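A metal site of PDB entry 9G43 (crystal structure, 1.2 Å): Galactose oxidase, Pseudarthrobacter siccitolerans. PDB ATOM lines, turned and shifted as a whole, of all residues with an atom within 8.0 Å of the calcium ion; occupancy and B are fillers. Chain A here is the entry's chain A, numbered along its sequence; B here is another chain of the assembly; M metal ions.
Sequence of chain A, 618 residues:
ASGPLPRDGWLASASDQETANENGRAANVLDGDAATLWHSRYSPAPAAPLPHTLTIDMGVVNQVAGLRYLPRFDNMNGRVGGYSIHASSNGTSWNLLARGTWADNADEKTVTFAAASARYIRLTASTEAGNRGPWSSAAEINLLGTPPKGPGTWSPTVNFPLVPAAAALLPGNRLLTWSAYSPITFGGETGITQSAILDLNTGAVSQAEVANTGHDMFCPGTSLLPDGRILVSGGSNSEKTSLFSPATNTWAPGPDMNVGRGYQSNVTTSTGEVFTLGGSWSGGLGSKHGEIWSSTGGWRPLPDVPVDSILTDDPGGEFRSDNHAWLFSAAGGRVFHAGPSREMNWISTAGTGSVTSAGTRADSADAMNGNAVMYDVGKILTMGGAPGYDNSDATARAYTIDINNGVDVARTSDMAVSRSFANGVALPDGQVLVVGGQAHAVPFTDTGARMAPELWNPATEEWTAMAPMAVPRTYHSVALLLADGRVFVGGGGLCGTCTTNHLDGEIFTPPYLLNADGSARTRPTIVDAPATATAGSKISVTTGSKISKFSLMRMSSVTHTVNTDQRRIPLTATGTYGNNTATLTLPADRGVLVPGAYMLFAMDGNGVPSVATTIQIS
ND2 of Asn 28 sits close to O of Arg 25, at 3.5 Å.
N of Gly 32 lies within hydrogen-bond range of OE1 of Glu 140, 2.9 Å away.
The side-chain carboxylate (OE1) of Glu 140 lies within salt-bridge range of the guanidinium group (NH2) of Arg 7.
The side-chain carboxylate (OD1) of Asp 33 lies within hydrogen-bond range of the backbone NH (N) of Ala 35, 2.9 Å away.
OG of Ser 4 of chain B sits at hydrogen-bond distance from OD2 of Asp 33 (2.6 Å).
O of Leu 70 is in hydrogen-bond range of N of Ala 139 (2.8 Å).
ND2 of Asn 28 sits at hydrogen-bond distance from O of Leu 37 (2.9 Å).
The backbone carbonyl oxygen (O) of Glu 140 is in hydrogen-bond range of the backbone NH (N) of Leu 70 (2.9 Å).
Of the 23 residues printed, 6 come within 4 Å of the calcium ion.
The nearest printed residue that does not touch the calcium ion is Val 29 (4.4 Å).
The calcium ion is bound by the backbone carbonyl oxygen (O) of Asn 28, the backbone carbonyl oxygen (O) of Asp 33, the side-chain carboxylate (OE2) of Glu 140, the backbone carbonyl oxygen (O) of Ala 139, the side-chain hydroxyl (OG1) of Thr 36, the side-chain carboxylate (OD1) of Asp 31 and the backbone carbonyl oxygen (O) of Thr 36.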
ATOM      1  N   ARG A   7     -22.378  19.297  23.282  1.00  0.00           N
ATOM      2  CA  ARG A   7     -21.631  20.453  22.826  1.00  0.00           C
ATOM      3  C   ARG A   7     -21.798  20.715  21.334  1.00  0.00           C
ATOM      4  O   ARG A   7     -21.151  21.609  20.779  1.00  0.00           O
ATOM      5  CB  ARG A   7     -20.140  20.294  23.181  1.00  0.00           C
ATOM      6  CG  ARG A   7     -19.925  20.126  24.675  1.00  0.00           C
ATOM      7  CD  ARG A   7     -18.497  20.329  25.111  1.00  0.00           C
ATOM      8  NE  ARG A   7     -17.639  19.326  24.473  1.00  0.00           N
ATOM      9  CZ  ARG A   7     -16.324  19.315  24.569  1.00  0.00           C
ATOM     10  NH1 ARG A   7     -15.723  20.259  25.284  1.00  0.00           N
ATOM     11  NH2 ARG A   7     -15.639  18.357  23.947  1.00  0.00           N
ATOM     12  N   ARG A  25      -5.930  28.067  19.631  1.00  0.00           N
ATOM     13  CA  ARG A  25      -7.232  28.616  19.309  1.00  0.00           C
ATOM     14  C   ARG A  25      -8.301  28.216  20.323  1.00  0.00           C
ATOM     15  O   ARG A  25      -8.339  27.092  20.822  1.00  0.00           O
ATOM     16  CB  ARG A  25      -7.656  28.212  17.904  1.00  0.00           C
ATOM     17  CG  ARG A  25      -6.835  28.869  16.804  1.00  0.00           C
ATOM     18  CD  ARG A  25      -7.211  28.450  15.389  1.00  0.00           C
ATOM     19  NE  ARG A  25      -6.528  29.323  14.423  1.00  0.00           N
ATOM     20  CZ  ARG A  25      -5.403  28.989  13.804  1.00  0.00           C
ATOM     21  NH1 ARG A  25      -4.849  27.808  14.014  1.00  0.00           N
ATOM     22  NH2 ARG A  25      -4.835  29.832  12.953  1.00  0.00           N
ATOM     23  N   ALA A  26      -9.210  29.165  20.592  1.00  0.00           N
ATOM     24  CA  ALA A  26     -10.292  28.977  21.563  1.00  0.00           C
ATOM     25  C   ALA A  26     -11.130  27.721  21.234  1.00  0.00           C
ATOM     26  O   ALA A  26     -11.541  27.023  22.156  1.00  0.00           O
ATOM     27  CB  ALA A  26     -11.210  30.211  21.551  1.00  0.00           C
ATOM     28  N   ALA A  27     -11.373  27.460  19.933  1.00  0.00           N
ATOM     29  CA  ALA A  27     -12.200  26.326  19.525  1.00  0.00           C
ATOM     30  C   ALA A  27     -11.651  25.016  20.095  1.00  0.00           C
ATOM     31  O   ALA A  27     -12.370  24.012  20.158  1.00  0.00           O
ATOM     32  CB  ALA A  27     -12.360  26.225  18.019  1.00  0.00           C
ATOM     33  N   ASN A  28     -10.344  24.967  20.410  1.00  0.00           N
ATOM     34  CA  ASN A  28      -9.708  23.737  20.845  1.00  0.00           C
ATOM     35  C   ASN A  28     -10.273  23.250  22.181  1.00  0.00           C
ATOM     36  O   ASN A  28     -10.015  22.090  22.523  1.00  0.00           O
ATOM     37  CB  ASN A  28      -8.180  23.880  20.927  1.00  0.00           C
ATOM     38  CG  ASN A  28      -7.526  24.076  19.576  1.00  0.00           C
ATOM     39  OD1 ASN A  28      -8.133  23.807  18.538  1.00  0.00           O
ATOM     40  ND2 ASN A  28      -6.283  24.549  19.579  1.00  0.00           N
ATOM     41  N   VAL A  29     -11.027  24.084  22.926  1.00  0.00           N
ATOM     42  CA  VAL A  29     -11.593  23.588  24.186  1.00  0.00           C
ATOM     43  C   VAL A  29     -12.831  22.741  23.935  1.00  0.00           C
ATOM     44  O   VAL A  29     -13.332  22.157  24.913  1.00  0.00           O
ATOM     45  CB  VAL A  29     -11.900  24.682  25.226  1.00  0.00           C
ATOM     46  CG1 VAL A  29     -10.656  25.556  25.495  1.00  0.00           C
ATOM     47  CG2 VAL A  29     -13.103  25.552  24.810  1.00  0.00           C
ATOM     48  N   LEU A  30     -13.310  22.647  22.670  1.00  0.00           N
ATOM     49  CA  LEU A  30     -14.597  22.009  22.382  1.00  0.00           C
ATOM     50  C   LEU A  30     -14.445  20.755  21.540  1.00  0.00           C
ATOM     51  O   LEU A  30     -15.462  20.209  21.099  1.00  0.00           O
ATOM     52  CB  LEU A  30     -15.483  22.998  21.586  1.00  0.00           C
ATOM     53  CG  LEU A  30     -15.865  24.274  22.336  1.00  0.00           C
ATOM     54  CD1 LEU A  30     -16.717  25.214  21.476  1.00  0.00           C
ATOM     55  CD2 LEU A  30     -16.555  23.950  23.655  1.00  0.00           C
ATOM     56  N   ASP A  31     -13.228  20.297  21.262  1.00  0.00           N
ATOM     57  CA  ASP A  31     -13.017  19.231  20.283  1.00  0.00           C
ATOM     58  C   ASP A  31     -12.973  17.861  20.927  1.00  0.00           C
ATOM     59  O   ASP A  31     -12.987  16.875  20.200  1.00  0.00           O
ATOM     60  CB  ASP A  31     -11.820  19.482  19.375  1.00  0.00           C
ATOM     61  CG  ASP A  31     -10.485  19.612  20.104  1.00  0.00           C
ATOM     62  OD1 ASP A  31     -10.440  19.376  21.339  1.00  0.00           O
ATOM     63  OD2 ASP A  31      -9.480  19.941  19.429  1.00  0.00           O
ATOM     64  N   GLY A  32     -12.945  17.772  22.268  1.00  0.00           N
ATOM     65  CA  GLY A  32     -12.847  16.485  22.932  1.00  0.00           C
ATOM     66  C   GLY A  32     -11.409  15.970  23.059  1.00  0.00           C
ATOM     67  O   GLY A  32     -11.187  14.975  23.729  1.00  0.00           O
ATOM     68  N   ASP A  33     -10.436  16.693  22.457  1.00  0.00           N
ATOM     69  CA  ASP A  33      -9.070  16.234  22.425  1.00  0.00           C
ATOM     70  C   ASP A  33      -8.304  16.832  23.610  1.00  0.00           C
ATOM     71  O   ASP A  33      -8.134  18.056  23.690  1.00  0.00           O
ATOM     72  CB  ASP A  33      -8.477  16.635  21.066  1.00  0.00           C
ATOM     73  CG  ASP A  33      -7.129  16.034  20.738  1.00  0.00           C
ATOM     74  OD1 ASP A  33      -6.394  15.601  21.653  1.00  0.00           O
ATOM     75  OD2 ASP A  33      -6.832  15.983  19.537  1.00  0.00           O
ATOM     76  N   ALA A  34      -7.843  15.965  24.491  1.00  0.00           N
ATOM     77  CA  ALA A  34      -7.036  16.388  25.639  1.00  0.00           C
ATOM     78  C   ALA A  34      -5.701  17.021  25.248  1.00  0.00           C
ATOM     79  O   ALA A  34      -5.068  17.694  26.095  1.00  0.00           O
ATOM     80  CB  ALA A  34      -6.812  15.193  26.575  1.00  0.00           C
ATOM     81  N   ALA A  35      -5.244  16.794  24.002  1.00  0.00           N
ATOM     82  CA  ALA A  35      -3.941  17.285  23.576  1.00  0.00           C
ATOM     83  C   ALA A  35      -4.055  18.629  22.853  1.00  0.00           C
ATOM     84  O   ALA A  35      -3.011  19.203  22.529  1.00  0.00           O
ATOM     85  CB  ALA A  35      -3.280  16.249  22.665  1.00  0.00           C
ATOM     86  N   THR A  36      -5.280  19.143  22.592  1.00  0.00           N
ATOM     87  CA  THR A  36      -5.403  20.446  21.929  1.00  0.00           C
ATOM     88  C   THR A  36      -5.889  21.465  22.948  1.00  0.00           C
ATOM     89  O   THR A  36      -6.828  21.194  23.689  1.00  0.00           O
ATOM     90  CB  THR A  36      -6.337  20.395  20.712  1.00  0.00           C
ATOM     91  OG1 THR A  36      -7.660  20.074  21.187  1.00  0.00           O
ATOM     92  CG2 THR A  36      -5.872  19.425  19.632  1.00  0.00           C
ATOM     93  N   LEU A  37      -5.281  22.662  22.931  1.00  0.00           N
ATOM     94  CA  LEU A  37      -5.563  23.666  23.968  1.00  0.00           C
ATOM     95  C   LEU A  37      -6.005  24.980  23.369  1.00  0.00           C
ATOM     96  O   LEU A  37      -5.567  25.346  22.277  1.00  0.00           O
ATOM     97  CB  LEU A  37      -4.265  23.996  24.731  1.00  0.00           C
ATOM     98  CG  LEU A  37      -3.318  22.876  25.096  1.00  0.00           C
ATOM     99  CD1 LEU A  37      -2.120  23.487  25.817  1.00  0.00           C
ATOM    100  CD2 LEU A  37      -4.068  21.942  26.005  1.00  0.00           C
ATOM    101  N   TRP A  38      -6.851  25.703  24.134  1.00  0.00           N
ATOM    102  CA  TRP A  38      -6.802  27.163  24.094  1.00  0.00           C
ATOM    103  C   TRP A  38      -5.604  27.588  24.948  1.00  0.00           C
ATOM    104  O   TRP A  38      -5.414  27.087  26.067  1.00  0.00           O
ATOM    105  CB  TRP A  38      -8.082  27.765  24.671  1.00  0.00           C
ATOM    106  CG  TRP A  38      -7.975  29.245  24.916  1.00  0.00           C
ATOM    107  CD1 TRP A  38      -7.685  30.220  24.001  1.00  0.00           C
ATOM    108  CD2 TRP A  38      -8.122  29.884  26.193  1.00  0.00           C
ATOM    109  NE1 TRP A  38      -7.702  31.451  24.630  1.00  0.00           N
ATOM    110  CE2 TRP A  38      -7.933  31.270  25.967  1.00  0.00           C
ATOM    111  CE3 TRP A  38      -8.388  29.426  27.496  1.00  0.00           C
ATOM    112  CZ2 TRP A  38      -8.035  32.200  27.021  1.00  0.00           C
ATOM    113  CZ3 TRP A  38      -8.485  30.347  28.528  1.00  0.00           C
ATOM    114  CH2 TRP A  38      -8.332  31.718  28.273  1.00  0.00           C
ATOM    115  N   LEU A  70     -10.589  21.070  32.083  1.00  0.00           N
ATOM    116  CA  LEU A  70      -9.522  20.066  31.991  1.00  0.00           C
ATOM    117  C   LEU A  70      -8.238  20.805  31.606  1.00  0.00           C
ATOM    118  O   LEU A  70      -8.132  21.376  30.519  1.00  0.00           O
ATOM    119  CB  LEU A  70      -9.861  19.023  30.908  1.00  0.00           C
ATOM    120  CG  LEU A  70      -8.792  17.955  30.746  1.00  0.00           C
ATOM    121  CD1 LEU A  70      -8.858  16.966  31.912  1.00  0.00           C
ATOM    122  CD2 LEU A  70      -9.055  17.236  29.400  1.00  0.00           C
ATOM    123  N   ALA A 138      -6.361  25.836  28.487  1.00  0.00           N
ATOM    124  CA  ALA A 138      -7.387  24.852  28.838  1.00  0.00           C
ATOM    125  C   ALA A 138      -7.425  23.841  27.712  1.00  0.00           C
ATOM    126  O   ALA A 138      -7.469  24.242  26.537  1.00  0.00           O
ATOM    127  CB  ALA A 138      -8.753  25.548  28.941  1.00  0.00           C
ATOM    128  N   ALA A 139      -7.429  22.543  28.079  1.00  0.00           N
ATOM    129  CA  ALA A 139      -7.539  21.519  27.047  1.00  0.00           C
ATOM    130  C   ALA A 139      -8.993  21.307  26.649  1.00  0.00           C
ATOM    131  O   ALA A 139      -9.270  21.071  25.478  1.00  0.00           O
ATOM    132  CB  ALA A 139      -6.906  20.237  27.561  1.00  0.00           C
ATOM    133  N   GLU A 140      -9.898  21.323  27.637  1.00  0.00           N
ATOM    134  CA  GLU A 140     -11.319  21.053  27.371  1.00  0.00           C
ATOM    135  C   GLU A 140     -12.143  21.817  28.392  1.00  0.00           C
ATOM    136  O   GLU A 140     -11.730  21.968  29.552  1.00  0.00           O
ATOM    137  CB  GLU A 140     -11.653  19.557  27.538  1.00  0.00           C
ATOM    138  CG  GLU A 140     -11.120  18.703  26.395  1.00  0.00           C
ATOM    139  CD  GLU A 140     -11.801  18.958  25.055  1.00  0.00           C
ATOM    140  OE1 GLU A 140     -13.043  18.812  25.014  1.00  0.00           O
ATOM    141  OE2 GLU A 140     -11.097  19.302  24.059  1.00  0.00           O
ATOM    142  N   ILE A 141     -13.296  22.336  27.951  1.00  0.00           N
ATOM    143  CA  ILE A 141     -14.258  22.909  28.890  1.00  0.00           C
ATOM    144  C   ILE A 141     -15.608  22.287  28.569  1.00  0.00           C
ATOM    145  O   ILE A 141     -16.044  22.325  27.410  1.00  0.00           O
ATOM    146  CB  ILE A 141     -14.336  24.452  28.819  1.00  0.00           C
ATOM    147  CG1 ILE A 141     -12.988  25.084  29.185  1.00  0.00           C
ATOM    148  CG2 ILE A 141     -15.448  24.960  29.722  1.00  0.00           C
ATOM    149  CD1 ILE A 141     -12.950  26.597  28.886  1.00  0.00           C
ATOM    150  N   SER B   1     -13.226  11.994  26.941  1.00  0.00           N
ATOM    151  CA  SER B   1     -12.233  12.703  26.106  1.00  0.00           C
ATOM    152  C   SER B   1     -11.409  11.687  25.292  1.00  0.00           C
ATOM    153  O   SER B   1     -11.386  10.497  25.589  1.00  0.00           O
ATOM    154  CB  SER B   1     -11.347  13.648  26.956  1.00  0.00           C
ATOM    155  OG  SER B   1     -10.460  12.950  27.840  1.00  0.00           O
ATOM    156  N   HIS B   2     -10.743  12.166  24.238  1.00  0.00           N
ATOM    157  CA  HIS B   2      -9.752  11.383  23.544  1.00  0.00           C
ATOM    158  C   HIS B   2      -8.475  12.211  23.541  1.00  0.00           C
ATOM    159  O   HIS B   2      -8.451  13.307  24.123  1.00  0.00           O
ATOM    160  CB  HIS B   2     -10.239  11.089  22.123  1.00  0.00           C
ATOM    161  CG  HIS B   2     -10.459  12.283  21.250  1.00  0.00           C
ATOM    162  ND1 HIS B   2     -11.623  13.027  21.273  1.00  0.00           N
ATOM    163  CD2 HIS B   2      -9.673  12.846  20.296  1.00  0.00           C
ATOM    164  CE1 HIS B   2     -11.527  14.027  20.397  1.00  0.00           C
ATOM    165  NE2 HIS B   2     -10.363  13.944  19.774  1.00  0.00           N
ATOM    166  N   SER B   4      -5.063  13.114  20.664  1.00  0.00           N
ATOM    167  CA  SER B   4      -4.289  12.917  19.450  1.00  0.00           C
ATOM    168  C   SER B   4      -2.810  12.877  19.776  1.00  0.00           C
ATOM    169  O   SER B   4      -2.016  12.616  18.870  1.00  0.00           O
ATOM    170  CB  SER B   4      -4.598  13.991  18.416  1.00  0.00           C
ATOM    171  OG  SER B   4      -4.410  15.297  18.953  1.00  0.00           O
HETATM  172 CA    CA M   1      -9.048  20.164  23.236  1.00  0.00          CA
